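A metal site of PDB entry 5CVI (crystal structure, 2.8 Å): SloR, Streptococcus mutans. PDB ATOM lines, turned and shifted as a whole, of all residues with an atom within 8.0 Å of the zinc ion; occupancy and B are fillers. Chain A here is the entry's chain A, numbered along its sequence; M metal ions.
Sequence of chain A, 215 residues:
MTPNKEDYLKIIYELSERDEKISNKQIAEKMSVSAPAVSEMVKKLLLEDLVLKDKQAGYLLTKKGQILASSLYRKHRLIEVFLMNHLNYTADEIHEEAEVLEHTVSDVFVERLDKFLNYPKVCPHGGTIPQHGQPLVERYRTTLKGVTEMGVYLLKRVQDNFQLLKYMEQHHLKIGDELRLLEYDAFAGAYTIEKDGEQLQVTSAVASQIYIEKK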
ATOM      1  N   PRO A   3       9.072   0.137  -4.927  1.00  0.00           N
ATOM      2  CA  PRO A   3       9.720  -1.032  -4.319  1.00  0.00           C
ATOM      3  C   PRO A   3       8.837  -2.271  -4.400  1.00  0.00           C
ATOM      4  O   PRO A   3       7.840  -2.351  -3.675  1.00  0.00           O
ATOM      5  CB  PRO A   3       9.896  -0.616  -2.856  1.00  0.00           C
ATOM      6  CG  PRO A   3       9.871   0.866  -2.869  1.00  0.00           C
ATOM      7  CD  PRO A   3       8.920   1.245  -3.968  1.00  0.00           C
ATOM      8  N   ASN A   4       9.193  -3.224  -5.254  1.00  0.00           N
ATOM      9  CA  ASN A   4       8.402  -4.443  -5.417  1.00  0.00           C
ATOM     10  C   ASN A   4       8.484  -5.352  -4.188  1.00  0.00           C
ATOM     11  O   ASN A   4       9.176  -5.035  -3.216  1.00  0.00           O
ATOM     12  CB  ASN A   4       8.827  -5.202  -6.671  1.00  0.00           C
ATOM     13  CG  ASN A   4      10.274  -5.638  -6.623  1.00  0.00           C
ATOM     14  OD1 ASN A   4      11.113  -5.014  -5.973  1.00  0.00           O
ATOM     15  ND2 ASN A   4      10.588  -6.730  -7.330  1.00  0.00           N
ATOM     16  N   LYS A   5       7.767  -6.465  -4.232  1.00  0.00           N
ATOM     17  CA  LYS A   5       7.713  -7.390  -3.097  1.00  0.00           C
ATOM     18  C   LYS A   5       9.083  -7.918  -2.701  1.00  0.00           C
ATOM     19  O   LYS A   5       9.358  -8.137  -1.530  1.00  0.00           O
ATOM     20  CB  LYS A   5       6.765  -8.562  -3.397  1.00  0.00           C
ATOM     21  CG  LYS A   5       7.184  -9.411  -4.576  1.00  0.00           C
ATOM     22  CD  LYS A   5       6.353 -10.676  -4.696  1.00  0.00           C
ATOM     23  CE  LYS A   5       6.806 -11.507  -5.889  1.00  0.00           C
ATOM     24  NZ  LYS A   5       6.035 -12.764  -6.037  1.00  0.00           N
ATOM     25  N   GLU A   6       9.948  -8.115  -3.701  1.00  0.00           N
ATOM     26  CA  GLU A   6      11.277  -8.663  -3.463  1.00  0.00           C
ATOM     27  C   GLU A   6      12.116  -7.749  -2.580  1.00  0.00           C
ATOM     28  O   GLU A   6      13.020  -8.208  -1.874  1.00  0.00           O
ATOM     29  CB  GLU A   6      11.977  -8.934  -4.800  1.00  0.00           C
ATOM     30  CG  GLU A   6      11.255  -9.952  -5.666  1.00  0.00           C
ATOM     31  CD  GLU A   6      11.586  -9.818  -7.138  1.00  0.00           C
ATOM     32  OE1 GLU A   6      10.936  -8.994  -7.821  1.00  0.00           O
ATOM     33  OE2 GLU A   6      12.484 -10.544  -7.613  1.00  0.00           O
ATOM     34  N   ASP A   7      11.820  -6.452  -2.620  1.00  0.00           N
ATOM     35  CA  ASP A   7      12.519  -5.485  -1.785  1.00  0.00           C
ATOM     36  C   ASP A   7      12.203  -5.700  -0.312  1.00  0.00           C
ATOM     37  O   ASP A   7      13.058  -5.517   0.558  1.00  0.00           O
ATOM     38  CB  ASP A   7      12.161  -4.067  -2.202  1.00  0.00           C
ATOM     39  CG  ASP A   7      12.961  -3.593  -3.399  1.00  0.00           C
ATOM     40  OD1 ASP A   7      14.079  -4.112  -3.596  1.00  0.00           O
ATOM     41  OD2 ASP A   7      12.477  -2.709  -4.130  1.00  0.00           O
ATOM     42  N   TYR A   8      10.963  -6.095  -0.042  1.00  0.00           N
ATOM     43  CA  TYR A   8      10.499  -6.351   1.317  1.00  0.00           C
ATOM     44  C   TYR A   8      11.235  -7.538   1.943  1.00  0.00           C
ATOM     45  O   TYR A   8      11.440  -7.572   3.157  1.00  0.00           O
ATOM     46  CB  TYR A   8       8.988  -6.578   1.311  1.00  0.00           C
ATOM     47  CG  TYR A   8       8.189  -5.315   1.063  1.00  0.00           C
ATOM     48  CD1 TYR A   8       7.533  -4.677   2.107  1.00  0.00           C
ATOM     49  CD2 TYR A   8       8.119  -4.749  -0.202  1.00  0.00           C
ATOM     50  CE1 TYR A   8       6.816  -3.513   1.892  1.00  0.00           C
ATOM     51  CE2 TYR A   8       7.401  -3.585  -0.427  1.00  0.00           C
ATOM     52  CZ  TYR A   8       6.750  -2.978   0.624  1.00  0.00           C
ATOM     53  OH  TYR A   8       6.028  -1.828   0.408  1.00  0.00           O
ATOM     54  N   LYS A  10      14.437  -8.370   1.434  1.00  0.00           N
ATOM     55  CA  LYS A  10      15.739  -7.884   1.870  1.00  0.00           C
ATOM     56  C   LYS A  10      15.633  -7.110   3.174  1.00  0.00           C
ATOM     57  O   LYS A  10      16.565  -7.105   3.980  1.00  0.00           O
ATOM     58  CB  LYS A  10      16.390  -7.017   0.783  1.00  0.00           C
ATOM     59  CG  LYS A  10      16.697  -7.770  -0.505  1.00  0.00           C
ATOM     60  CD  LYS A  10      17.593  -6.968  -1.428  1.00  0.00           C
ATOM     61  CE  LYS A  10      16.948  -5.638  -1.823  1.00  0.00           C
ATOM     62  NZ  LYS A  10      17.896  -4.769  -2.576  1.00  0.00           N
ATOM     63  N   LEU A  72      19.074 -11.934  -4.874  1.00  0.00           N
ATOM     64  CA  LEU A  72      18.966 -10.480  -4.958  1.00  0.00           C
ATOM     65  C   LEU A  72      20.243  -9.789  -4.493  1.00  0.00           C
ATOM     66  O   LEU A  72      20.726  -8.876  -5.160  1.00  0.00           O
ATOM     67  CB  LEU A  72      17.768  -9.966  -4.154  1.00  0.00           C
ATOM     68  CG  LEU A  72      16.505  -9.635  -4.952  1.00  0.00           C
ATOM     69  CD1 LEU A  72      16.026  -8.224  -4.635  1.00  0.00           C
ATOM     70  CD2 LEU A  72      16.770  -9.793  -6.445  1.00  0.00           C
ATOM     71  N   HIS A  76      22.703  -7.445  -6.740  1.00  0.00           N
ATOM     72  CA  HIS A  76      22.963  -6.103  -6.224  1.00  0.00           C
ATOM     73  C   HIS A  76      24.446  -5.847  -6.030  1.00  0.00           C
ATOM     74  O   HIS A  76      24.962  -4.808  -6.450  1.00  0.00           O
ATOM     75  CB  HIS A  76      22.223  -5.915  -4.897  1.00  0.00           C
ATOM     76  CG  HIS A  76      22.097  -4.480  -4.485  1.00  0.00           C
ATOM     77  ND1 HIS A  76      21.118  -3.650  -4.992  1.00  0.00           N
ATOM     78  CD2 HIS A  76      22.804  -3.736  -3.606  1.00  0.00           C
ATOM     79  CE1 HIS A  76      21.247  -2.449  -4.448  1.00  0.00           C
ATOM     80  NE2 HIS A  76      22.255  -2.481  -3.605  1.00  0.00           N
ATOM     81  N   HIS A  95      23.447   2.979  -5.075  1.00  0.00           N
ATOM     82  CA  HIS A  95      22.284   2.219  -4.629  1.00  0.00           C
ATOM     83  C   HIS A  95      21.124   2.213  -5.617  1.00  0.00           C
ATOM     84  O   HIS A  95      20.708   1.148  -6.082  1.00  0.00           O
ATOM     85  CB  HIS A  95      21.785   2.664  -3.256  1.00  0.00           C
ATOM     86  CG  HIS A  95      20.646   1.840  -2.747  1.00  0.00           C
ATOM     87  ND1 HIS A  95      20.797   0.516  -2.407  1.00  0.00           N
ATOM     88  CD2 HIS A  95      19.342   2.142  -2.541  1.00  0.00           C
ATOM     89  CE1 HIS A  95      19.635   0.028  -2.012  1.00  0.00           C
ATOM     90  NE2 HIS A  95      18.735   1.001  -2.075  1.00  0.00           N
ATOM     91  N   ALA A  98      21.980   0.374  -8.776  1.00  0.00           N
ATOM     92  CA  ALA A  98      22.062  -1.066  -8.545  1.00  0.00           C
ATOM     93  C   ALA A  98      20.692  -1.641  -8.200  1.00  0.00           C
ATOM     94  O   ALA A  98      20.406  -2.797  -8.457  1.00  0.00           O
ATOM     95  CB  ALA A  98      23.058  -1.371  -7.436  1.00  0.00           C
ATOM     96  N   GLU A  99      19.864  -0.800  -7.605  1.00  0.00           N
ATOM     97  CA  GLU A  99      18.520  -1.182  -7.209  1.00  0.00           C
ATOM     98  C   GLU A  99      17.642  -1.439  -8.424  1.00  0.00           C
ATOM     99  O   GLU A  99      16.904  -2.431  -8.457  1.00  0.00           O
ATOM    100  CB  GLU A  99      17.897  -0.076  -6.328  1.00  0.00           C
ATOM    101  CG  GLU A  99      16.493  -0.361  -5.867  1.00  0.00           C
ATOM    102  CD  GLU A  99      16.362  -1.730  -5.229  1.00  0.00           C
ATOM    103  OE1 GLU A  99      17.327  -2.158  -4.549  1.00  0.00           O
ATOM    104  OE2 GLU A  99      15.314  -2.376  -5.418  1.00  0.00           O
ATOM    105  N   VAL A 100      17.734  -0.562  -9.406  1.00  0.00           N
ATOM    106  CA  VAL A 100      16.970  -0.710 -10.639  1.00  0.00           C
ATOM    107  C   VAL A 100      17.436  -1.917 -11.455  1.00  0.00           C
ATOM    108  O   VAL A 100      16.615  -2.710 -11.938  1.00  0.00           O
ATOM    109  CB  VAL A 100      17.039   0.573 -11.508  1.00  0.00           C
ATOM    110  CG1 VAL A 100      16.875   0.250 -12.975  1.00  0.00           C
ATOM    111  CG2 VAL A 100      15.989   1.575 -11.052  1.00  0.00           C
ATOM    112  N   LEU A 101      18.750  -2.058 -11.591  1.00  0.00           N
ATOM    113  CA  LEU A 101      19.335  -3.113 -12.402  1.00  0.00           C
ATOM    114  C   LEU A 101      19.092  -4.528 -11.883  1.00  0.00           C
ATOM    115  O   LEU A 101      18.952  -5.471 -12.670  1.00  0.00           O
ATOM    116  CB  LEU A 101      20.848  -2.883 -12.578  1.00  0.00           C
ATOM    117  CG  LEU A 101      21.252  -1.701 -13.458  1.00  0.00           C
ATOM    118  CD1 LEU A 101      22.761  -1.614 -13.574  1.00  0.00           C
ATOM    119  CD2 LEU A 101      20.618  -1.850 -14.830  1.00  0.00           C
ATOM    120  N   GLU A 102      19.045  -4.690 -10.564  1.00  0.00           N
ATOM    121  CA  GLU A 102      18.857  -6.014  -9.965  1.00  0.00           C
ATOM    122  C   GLU A 102      17.465  -6.573 -10.314  1.00  0.00           C
ATOM    123  O   GLU A 102      17.246  -7.777 -10.229  1.00  0.00           O
ATOM    124  CB  GLU A 102      19.046  -5.973  -8.450  1.00  0.00           C
ATOM    125  CG  GLU A 102      17.859  -5.394  -7.683  1.00  0.00           C
ATOM    126  CD  GLU A 102      18.026  -5.474  -6.174  1.00  0.00           C
ATOM    127  OE1 GLU A 102      19.142  -5.772  -5.708  1.00  0.00           O
ATOM    128  OE2 GLU A 102      17.027  -5.244  -5.467  1.00  0.00           O
ATOM    129  N   HIS A 103      16.553  -5.695 -10.706  1.00  0.00           N
ATOM    130  CA  HIS A 103      15.204  -6.112 -11.070  1.00  0.00           C
ATOM    131  C   HIS A 103      14.996  -6.161 -12.583  1.00  0.00           C
ATOM    132  O   HIS A 103      13.902  -6.459 -13.055  1.00  0.00           O
ATOM    133  CB  HIS A 103      14.172  -5.181 -10.431  1.00  0.00           C
ATOM    134  CG  HIS A 103      14.137  -5.260  -8.945  1.00  0.00           C
ATOM    135  ND1 HIS A 103      13.820  -6.409  -8.266  1.00  0.00           N
ATOM    136  CD2 HIS A 103      14.385  -4.322  -8.001  1.00  0.00           C
ATOM    137  CE1 HIS A 103      13.869  -6.183  -6.962  1.00  0.00           C
ATOM    138  NE2 HIS A 103      14.208  -4.917  -6.776  1.00  0.00           N
HETATM  139 ZN    ZN M   1      15.293  -4.307  -5.178  1.00  0.00          ZN
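The zinc ion is bound by OE2 of Glu 99 (1.9 Å), OE2 of Glu 102 (2.0 Å), OD1 of Asp 7 (2.0 Å) and NE2 of His 103 (2.0 Å).
The zinc ion has four donor atoms within binding distance.
Merely in contact with the zinc ion: Lys 10.
Within 4 Å of the zinc ion: Asp 7, Lys 10, Glu 99, Glu 102 and His 103.
The side-chain carboxylate of Glu 99 is in salt-bridge range of the side-chain amino group of Lys 10.
The side-chain amino group (NZ) of Lys 10 lies within salt-bridge range of the side-chain carboxylate (OE1) of Glu 102.
The side-chain carboxylate of Glu 102 sits at hydrogen-bond distance from a ring nitrogen (ND1) of His 76, at 3.0 Å.
The side-chain carboxylate (OD2) of Asp 7 sits close to the side-chain amide oxygen (OD1) of Asn 4 (3.3 Å).
A ring nitrogen (ND1) of His 103 lies close to the side-chain amide nitrogen (ND2) of Asn 4.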
